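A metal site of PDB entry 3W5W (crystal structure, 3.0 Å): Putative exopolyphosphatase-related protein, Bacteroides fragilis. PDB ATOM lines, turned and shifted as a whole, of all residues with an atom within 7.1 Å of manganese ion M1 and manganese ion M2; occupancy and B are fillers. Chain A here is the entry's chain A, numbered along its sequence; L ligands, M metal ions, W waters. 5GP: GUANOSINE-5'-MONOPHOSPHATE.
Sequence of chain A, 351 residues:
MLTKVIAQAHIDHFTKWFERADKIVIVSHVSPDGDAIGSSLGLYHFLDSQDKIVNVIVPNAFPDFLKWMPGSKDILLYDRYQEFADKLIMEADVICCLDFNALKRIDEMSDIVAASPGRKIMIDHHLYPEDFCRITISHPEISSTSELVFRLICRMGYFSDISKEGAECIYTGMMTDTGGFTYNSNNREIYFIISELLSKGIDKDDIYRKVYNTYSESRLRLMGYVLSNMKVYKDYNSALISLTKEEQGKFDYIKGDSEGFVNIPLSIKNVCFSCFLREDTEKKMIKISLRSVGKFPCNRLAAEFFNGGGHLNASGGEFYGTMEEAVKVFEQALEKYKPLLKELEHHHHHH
Manganese ion M1 is bound by OD2 of Asp 35 (2.2 Å), OD1 of Asp 99 (2.2 Å), OD2 of Asp 177 (2.2 Å) and NE2 of His 125 (2.3 Å).
Manganese ion M1 has four donor atoms within binding distance.
The side-chain hydroxyl of Ser 146 lies within hydrogen-bond range of the side-chain carboxylate of Asp 35.
A ring nitrogen (ND1) of His 126 sits close to a ring nitrogen (NE2) of His 311 (3.3 Å).
ND1 of His 29 sits close to O of Ser 31, at 3.5 Å.
A ring nitrogen (ND1) of His 125 is in hydrogen-bond range of the backbone NH (N) of Ser 144, at 3.4 Å.
The backbone NH of His 126 sits at hydrogen-bond distance from the side-chain carboxylate of Asp 124 (2.7 Å).
OG1 of Thr 145 sits close to N of Asp 99, 3.4 Å away.
The backbone NH (N) of Asp 35 is in hydrogen-bond range of the side-chain carboxylate (OD2) of Asp 33, 3.2 Å away.
OD1 of Asp 35 sits at hydrogen-bond distance from N of Thr 145, at 3.3 Å.
O2' of the ligand lies within hydrogen-bond range of NH1 of Arg 105, 3.1 Å away.
Residues that only touch manganese ion M1: His 126 (3.7 Å).
Along chain A the residues within 4 Å of manganese ion M1 span positions 35 to 177.
The nearest printed residue that does not touch manganese ion M1 is Thr 145 (4.05 Å).
Of the 25 residues printed, 3 come within 4 Å of manganese ion M2.
The nearest printed residue that does not touch manganese ion M2 is Asp 35 (4.3 Å).
Manganese ion M2 is bound by the side-chain carboxylate (OD1) of Asp 33, the side-chain carboxylate (OD2) of Asp 99 and a ring nitrogen (NE2) of His 29.
Manganese ion M2 has three donor atoms within binding distance.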
ATOM      1  N   SER A  28      -0.414  -4.148   6.282  1.00  0.00           N
ATOM      2  CA  SER A  28      -0.735  -3.757   7.654  1.00  0.00           C
ATOM      3  C   SER A  28       0.473  -3.017   8.260  1.00  0.00           C
ATOM      4  O   SER A  28       1.524  -2.967   7.644  1.00  0.00           O
ATOM      5  CB  SER A  28      -1.119  -4.964   8.503  1.00  0.00           C
ATOM      6  OG  SER A  28      -1.705  -4.559   9.724  1.00  0.00           O
ATOM      7  N   HIS A  29       0.320  -2.471   9.472  1.00  0.00           N
ATOM      8  CA  HIS A  29       1.370  -1.669  10.107  1.00  0.00           C
ATOM      9  C   HIS A  29       2.625  -2.360  10.641  1.00  0.00           C
ATOM     10  O   HIS A  29       2.608  -3.544  10.961  1.00  0.00           O
ATOM     11  CB  HIS A  29       0.759  -0.832  11.231  1.00  0.00           C
ATOM     12  CG  HIS A  29       0.248  -1.650  12.374  1.00  0.00           C
ATOM     13  ND1 HIS A  29       1.082  -2.188  13.333  1.00  0.00           N
ATOM     14  CD2 HIS A  29      -1.003  -2.030  12.709  1.00  0.00           C
ATOM     15  CE1 HIS A  29       0.363  -2.854  14.219  1.00  0.00           C
ATOM     16  NE2 HIS A  29      -0.911  -2.787  13.862  1.00  0.00           N
ATOM     17  N   SER A  31       5.452  -3.849  12.920  1.00  0.00           N
ATOM     18  CA  SER A  31       5.229  -4.557  14.176  1.00  0.00           C
ATOM     19  C   SER A  31       3.770  -4.995  14.227  1.00  0.00           C
ATOM     20  O   SER A  31       2.979  -4.537  15.057  1.00  0.00           O
ATOM     21  CB  SER A  31       5.525  -3.659  15.379  1.00  0.00           C
ATOM     22  OG  SER A  31       6.916  -3.438  15.492  1.00  0.00           O
ATOM     23  N   PRO A  32       3.376  -5.883  13.316  1.00  0.00           N
ATOM     24  CA  PRO A  32       1.995  -6.359  13.292  1.00  0.00           C
ATOM     25  C   PRO A  32       1.632  -7.032  14.604  1.00  0.00           C
ATOM     26  O   PRO A  32       2.414  -7.823  15.157  1.00  0.00           O
ATOM     27  CB  PRO A  32       1.989  -7.345  12.123  1.00  0.00           C
ATOM     28  CG  PRO A  32       3.102  -6.867  11.259  1.00  0.00           C
ATOM     29  CD  PRO A  32       4.164  -6.530  12.254  1.00  0.00           C
ATOM     30  N   ASP A  33       0.445  -6.717  15.103  1.00  0.00           N
ATOM     31  CA  ASP A  33      -0.048  -7.307  16.332  1.00  0.00           C
ATOM     32  C   ASP A  33      -1.234  -8.182  15.948  1.00  0.00           C
ATOM     33  O   ASP A  33      -1.605  -8.255  14.774  1.00  0.00           O
ATOM     34  CB  ASP A  33      -0.521  -6.202  17.269  1.00  0.00           C
ATOM     35  CG  ASP A  33      -1.621  -5.359  16.675  1.00  0.00           C
ATOM     36  OD1 ASP A  33      -1.346  -4.552  15.779  1.00  0.00           O
ATOM     37  OD2 ASP A  33      -2.791  -5.533  17.095  1.00  0.00           O
ATOM     38  N   GLY A  34      -1.815  -8.848  16.938  1.00  0.00           N
ATOM     39  CA  GLY A  34      -2.958  -9.719  16.698  1.00  0.00           C
ATOM     40  C   GLY A  34      -4.031  -9.207  15.741  1.00  0.00           C
ATOM     41  O   GLY A  34      -4.499  -9.947  14.872  1.00  0.00           O
ATOM     42  N   ASP A  35      -4.422  -7.943  15.879  1.00  0.00           N
ATOM     43  CA  ASP A  35      -5.452  -7.401  14.999  1.00  0.00           C
ATOM     44  C   ASP A  35      -4.898  -7.270  13.595  1.00  0.00           C
ATOM     45  O   ASP A  35      -5.577  -7.595  12.618  1.00  0.00           O
ATOM     46  CB  ASP A  35      -5.943  -6.043  15.513  1.00  0.00           C
ATOM     47  CG  ASP A  35      -7.241  -5.583  14.846  1.00  0.00           C
ATOM     48  OD1 ASP A  35      -8.037  -6.441  14.408  1.00  0.00           O
ATOM     49  OD2 ASP A  35      -7.470  -4.353  14.765  1.00  0.00           O
ATOM     50  N   ALA A  36      -3.655  -6.808  13.481  1.00  0.00           N
ATOM     51  CA  ALA A  36      -3.032  -6.636  12.171  1.00  0.00           C
ATOM     52  C   ALA A  36      -2.996  -7.949  11.381  1.00  0.00           C
ATOM     53  O   ALA A  36      -3.508  -8.017  10.268  1.00  0.00           O
ATOM     54  CB  ALA A  36      -1.629  -6.078  12.350  1.00  0.00           C
ATOM     55  N   ILE A  37      -2.397  -8.971  11.955  1.00  0.00           N
ATOM     56  CA  ILE A  37      -2.306 -10.278  11.297  1.00  0.00           C
ATOM     57  C   ILE A  37      -3.669 -10.966  11.119  1.00  0.00           C
ATOM     58  O   ILE A  37      -3.939 -11.573  10.083  1.00  0.00           O
ATOM     59  CB  ILE A  37      -1.372 -11.237  12.091  1.00  0.00           C
ATOM     60  CG1 ILE A  37       0.049 -10.670  12.113  1.00  0.00           C
ATOM     61  CG2 ILE A  37      -1.420 -12.648  11.477  1.00  0.00           C
ATOM     62  CD1 ILE A  37       0.572 -10.252  10.757  1.00  0.00           C
ATOM     63  N   SER A  39      -6.891  -9.600  11.016  1.00  0.00           N
ATOM     64  CA  SER A  39      -7.764  -8.931  10.056  1.00  0.00           C
ATOM     65  C   SER A  39      -7.279  -9.143   8.629  1.00  0.00           C
ATOM     66  O   SER A  39      -8.086  -9.240   7.696  1.00  0.00           O
ATOM     67  CB  SER A  39      -7.809  -7.440  10.333  1.00  0.00           C
ATOM     68  OG  SER A  39      -6.547  -6.862  10.063  1.00  0.00           O
ATOM     69  N   LEU A  98      -5.054  -2.339   6.035  1.00  0.00           N
ATOM     70  CA  LEU A  98      -5.793  -2.673   7.233  1.00  0.00           C
ATOM     71  C   LEU A  98      -5.103  -2.354   8.538  1.00  0.00           C
ATOM     72  O   LEU A  98      -3.914  -2.607   8.712  1.00  0.00           O
ATOM     73  CB  LEU A  98      -6.167  -4.155   7.218  1.00  0.00           C
ATOM     74  CG  LEU A  98      -7.394  -4.545   6.395  1.00  0.00           C
ATOM     75  CD1 LEU A  98      -7.200  -4.214   4.924  1.00  0.00           C
ATOM     76  CD2 LEU A  98      -7.641  -6.030   6.570  1.00  0.00           C
ATOM     77  N   ASP A  99      -5.863  -1.755   9.451  1.00  0.00           N
ATOM     78  CA  ASP A  99      -5.360  -1.461  10.776  1.00  0.00           C
ATOM     79  C   ASP A  99      -4.297  -0.363  10.953  1.00  0.00           C
ATOM     80  O   ASP A  99      -3.482  -0.425  11.883  1.00  0.00           O
ATOM     81  CB  ASP A  99      -4.892  -2.774  11.395  1.00  0.00           C
ATOM     82  CG  ASP A  99      -4.945  -2.752  12.888  1.00  0.00           C
ATOM     83  OD1 ASP A  99      -6.017  -2.441  13.430  1.00  0.00           O
ATOM     84  OD2 ASP A  99      -3.906  -3.056  13.504  1.00  0.00           O
ATOM     85  N   PHE A 100      -4.315   0.633  10.083  1.00  0.00           N
ATOM     86  CA  PHE A 100      -3.414   1.782  10.196  1.00  0.00           C
ATOM     87  C   PHE A 100      -4.021   2.851   9.311  1.00  0.00           C
ATOM     88  O   PHE A 100      -4.709   2.547   8.337  1.00  0.00           O
ATOM     89  CB  PHE A 100      -1.986   1.441   9.744  1.00  0.00           C
ATOM     90  CG  PHE A 100      -1.828   1.284   8.265  1.00  0.00           C
ATOM     91  CD1 PHE A 100      -2.093   0.074   7.639  1.00  0.00           C
ATOM     92  CD2 PHE A 100      -1.377   2.352   7.480  1.00  0.00           C
ATOM     93  CE1 PHE A 100      -1.915  -0.087   6.264  1.00  0.00           C
ATOM     94  CE2 PHE A 100      -1.191   2.199   6.099  1.00  0.00           C
ATOM     95  CZ  PHE A 100      -1.467   0.982   5.493  1.00  0.00           C
ATOM     96  N   ARG A 105       2.915   4.711   9.232  1.00  0.00           N
ATOM     97  CA  ARG A 105       2.696   3.497  10.004  1.00  0.00           C
ATOM     98  C   ARG A 105       3.272   2.236   9.386  1.00  0.00           C
ATOM     99  O   ARG A 105       3.635   1.299  10.102  1.00  0.00           O
ATOM    100  CB  ARG A 105       1.199   3.310  10.250  1.00  0.00           C
ATOM    101  CG  ARG A 105       0.618   4.314  11.230  1.00  0.00           C
ATOM    102  CD  ARG A 105       1.260   4.134  12.569  1.00  0.00           C
ATOM    103  NE  ARG A 105       0.952   2.820  13.097  1.00  0.00           N
ATOM    104  CZ  ARG A 105       1.708   2.197  13.994  1.00  0.00           C
ATOM    105  NH1 ARG A 105       2.806   2.776  14.440  1.00  0.00           N
ATOM    106  NH2 ARG A 105       1.360   0.989  14.431  1.00  0.00           N
ATOM    107  N   ASP A 124      -9.811   0.787   8.951  1.00  0.00           N
ATOM    108  CA  ASP A 124      -9.140   1.031  10.217  1.00  0.00           C
ATOM    109  C   ASP A 124     -10.077   1.517  11.321  1.00  0.00           C
ATOM    110  O   ASP A 124     -11.230   1.846  11.072  1.00  0.00           O
ATOM    111  CB  ASP A 124      -8.048   2.084  10.000  1.00  0.00           C
ATOM    112  CG  ASP A 124      -7.250   2.370  11.242  1.00  0.00           C
ATOM    113  OD1 ASP A 124      -6.659   1.409  11.786  1.00  0.00           O
ATOM    114  OD2 ASP A 124      -7.212   3.538  11.672  1.00  0.00           O
ATOM    115  N   HIS A 125      -9.557   1.578  12.552  1.00  0.00           N
ATOM    116  CA  HIS A 125     -10.340   2.048  13.686  1.00  0.00           C
ATOM    117  C   HIS A 125      -9.533   2.952  14.613  1.00  0.00           C
ATOM    118  O   HIS A 125      -9.866   3.112  15.785  1.00  0.00           O
ATOM    119  CB  HIS A 125     -10.895   0.873  14.508  1.00  0.00           C
ATOM    120  CG  HIS A 125      -9.848   0.055  15.177  1.00  0.00           C
ATOM    121  ND1 HIS A 125      -9.943  -0.361  16.487  1.00  0.00           N
ATOM    122  CD2 HIS A 125      -8.684  -0.461  14.711  1.00  0.00           C
ATOM    123  CE1 HIS A 125      -8.901  -1.093  16.798  1.00  0.00           C
ATOM    124  NE2 HIS A 125      -8.114  -1.182  15.737  1.00  0.00           N
ATOM    125  N   HIS A 126      -8.465   3.536  14.090  1.00  0.00           N
ATOM    126  CA  HIS A 126      -7.649   4.436  14.889  1.00  0.00           C
ATOM    127  C   HIS A 126      -8.125   5.869  14.616  1.00  0.00           C
ATOM    128  O   HIS A 126      -8.753   6.120  13.597  1.00  0.00           O
ATOM    129  CB  HIS A 126      -6.179   4.243  14.500  1.00  0.00           C
ATOM    130  CG  HIS A 126      -5.638   2.917  14.939  1.00  0.00           C
ATOM    131  ND1 HIS A 126      -5.091   2.708  16.185  1.00  0.00           N
ATOM    132  CD2 HIS A 126      -5.613   1.714  14.315  1.00  0.00           C
ATOM    133  CE1 HIS A 126      -4.764   1.432  16.319  1.00  0.00           C
ATOM    134  NE2 HIS A 126      -5.070   0.811  15.191  1.00  0.00           N
ATOM    135  N   SER A 143     -14.026  -1.568  18.107  1.00  0.00           N
ATOM    136  CA  SER A 143     -12.884  -2.144  18.823  1.00  0.00           C
ATOM    137  C   SER A 143     -11.727  -2.792  18.067  1.00  0.00           C
ATOM    138  O   SER A 143     -10.650  -2.958  18.652  1.00  0.00           O
ATOM    139  CB  SER A 143     -13.390  -3.137  19.879  1.00  0.00           C
ATOM    140  OG  SER A 143     -14.147  -4.177  19.281  1.00  0.00           O
ATOM    141  N   SER A 144     -11.918  -3.158  16.808  1.00  0.00           N
ATOM    142  CA  SER A 144     -10.839  -3.797  16.045  1.00  0.00           C
ATOM    143  C   SER A 144     -11.004  -3.672  14.539  1.00  0.00           C
ATOM    144  O   SER A 144     -12.092  -3.430  14.059  1.00  0.00           O
ATOM    145  CB  SER A 144     -10.781  -5.299  16.401  1.00  0.00           C
ATOM    146  OG  SER A 144     -11.979  -5.959  16.048  1.00  0.00           O
ATOM    147  N   THR A 145      -9.904  -3.847  13.806  1.00  0.00           N
ATOM    148  CA  THR A 145      -9.984  -3.789  12.352  1.00  0.00           C
ATOM    149  C   THR A 145     -10.615  -5.114  11.954  1.00  0.00           C
ATOM    150  O   THR A 145     -11.466  -5.166  11.059  1.00  0.00           O
ATOM    151  CB  THR A 145      -8.577  -3.641  11.695  1.00  0.00           C
ATOM    152  OG1 THR A 145      -8.063  -2.325  11.942  1.00  0.00           O
ATOM    153  CG2 THR A 145      -8.672  -3.834  10.188  1.00  0.00           C
ATOM    154  N   SER A 146     -10.221  -6.180  12.648  1.00  0.00           N
ATOM    155  CA  SER A 146     -10.771  -7.516  12.404  1.00  0.00           C
ATOM    156  C   SER A 146     -12.298  -7.518  12.341  1.00  0.00           C
ATOM    157  O   SER A 146     -12.902  -8.166  11.495  1.00  0.00           O
ATOM    158  CB  SER A 146     -10.337  -8.495  13.500  1.00  0.00           C
ATOM    159  OG  SER A 146      -8.937  -8.595  13.594  1.00  0.00           O
ATOM    160  N   GLY A 173      -8.030 -11.368  15.930  1.00  0.00           N
ATOM    161  CA  GLY A 173      -7.842  -9.932  15.850  1.00  0.00           C
ATOM    162  C   GLY A 173      -8.744  -9.188  16.837  1.00  0.00           C
ATOM    163  O   GLY A 173      -8.308  -8.228  17.472  1.00  0.00           O
ATOM    164  N   THR A 176      -7.505  -9.942  20.550  1.00  0.00           N
ATOM    165  CA  THR A 176      -6.292  -9.192  20.780  1.00  0.00           C
ATOM    166  C   THR A 176      -6.487  -7.713  21.081  1.00  0.00           C
ATOM    167  O   THR A 176      -5.942  -7.208  22.056  1.00  0.00           O
ATOM    168  CB  THR A 176      -5.364  -9.311  19.568  1.00  0.00           C
ATOM    169  OG1 THR A 176      -4.479 -10.409  19.776  1.00  0.00           O
ATOM    170  CG2 THR A 176      -4.556  -7.997  19.341  1.00  0.00           C
ATOM    171  N   ASP A 177      -7.235  -7.022  20.243  1.00  0.00           N
ATOM    172  CA  ASP A 177      -7.450  -5.592  20.437  1.00  0.00           C
ATOM    173  C   ASP A 177      -8.334  -5.207  21.599  1.00  0.00           C
ATOM    174  O   ASP A 177      -8.546  -4.031  21.859  1.00  0.00           O
ATOM    175  CB  ASP A 177      -7.968  -4.968  19.150  1.00  0.00           C
ATOM    176  CG  ASP A 177      -6.870  -4.284  18.361  1.00  0.00           C
ATOM    177  OD1 ASP A 177      -5.684  -4.664  18.520  1.00  0.00           O
ATOM    178  OD2 ASP A 177      -7.202  -3.372  17.573  1.00  0.00           O
ATOM    179  N   HIS A 311      -1.281   5.946  21.221  1.00  0.00           N
ATOM    180  CA  HIS A 311      -2.696   6.141  21.518  1.00  0.00           C
ATOM    181  C   HIS A 311      -2.953   6.568  22.956  1.00  0.00           C
ATOM    182  O   HIS A 311      -2.061   6.563  23.792  1.00  0.00           O
ATOM    183  CB  HIS A 311      -3.460   4.852  21.200  1.00  0.00           C
ATOM    184  CG  HIS A 311      -3.141   4.289  19.855  1.00  0.00           C
ATOM    185  ND1 HIS A 311      -3.243   5.019  18.696  1.00  0.00           N
ATOM    186  CD2 HIS A 311      -2.660   3.070  19.489  1.00  0.00           C
ATOM    187  CE1 HIS A 311      -2.838   4.286  17.675  1.00  0.00           C
ATOM    188  NE2 HIS A 311      -2.483   3.101  18.129  1.00  0.00           N
HETATM  189  P   5GP L   1       4.393  -0.357  23.105  1.00  0.00           P
HETATM  190  O1P 5GP L   1       4.057  -1.758  22.748  1.00  0.00           O
HETATM  191  O2P 5GP L   1       5.865   0.008  22.544  1.00  0.00           O
HETATM  192  O3P 5GP L   1       4.388  -0.191  24.706  1.00  0.00           O
HETATM  193  O5' 5GP L   1       3.288   0.652  22.469  1.00  0.00           O
HETATM  194  C5' 5GP L   1       3.309   0.493  21.044  1.00  0.00           C
HETATM  195  C4' 5GP L   1       2.296   1.440  20.388  1.00  0.00           C
HETATM  196  O4' 5GP L   1       2.597   2.831  20.718  1.00  0.00           O
HETATM  197  C3' 5GP L   1       2.320   1.285  18.855  1.00  0.00           C
HETATM  198  O3' 5GP L   1       1.025   0.929  18.348  1.00  0.00           O
HETATM  199  C2' 5GP L   1       2.813   2.637  18.291  1.00  0.00           C
HETATM  200  O2' 5GP L   1       1.862   3.205  17.394  1.00  0.00           O
HETATM  201  C1' 5GP L   1       3.058   3.545  19.520  1.00  0.00           C
HETATM  202  N9  5GP L   1       4.502   3.932  19.646  1.00  0.00           N
HETATM  203  C8  5GP L   1       5.476   3.263  20.356  1.00  0.00           C
HETATM  204  N7  5GP L   1       6.622   3.883  20.256  1.00  0.00           N
HETATM  205  C5  5GP L   1       6.465   4.983  19.479  1.00  0.00           C
HETATM  206  C6  5GP L   1       7.347   6.016  19.030  1.00  0.00           C
HETATM  207  O6  5GP L   1       8.523   6.021  19.354  1.00  0.00           O
HETATM  208  N1  5GP L   1       6.842   7.015  18.230  1.00  0.00           N
HETATM  209  C2  5GP L   1       5.507   7.020  17.862  1.00  0.00           C
HETATM  210  N2  5GP L   1       5.029   8.030  17.066  1.00  0.00           N
HETATM  211  N3  5GP L   1       4.675   6.061  18.283  1.00  0.00           N
HETATM  212  C4  5GP L   1       5.106   5.033  19.073  1.00  0.00           C
HETATM  213 MN    MN M   1      -6.393  -2.670  15.615  1.00  0.00          MN
HETATM  214 MN    MN M   2      -2.928  -2.981  15.533  1.00  0.00          MN
HETATM  215  O   HOH W   1      -4.590  -1.506  17.997  1.00  0.00           O
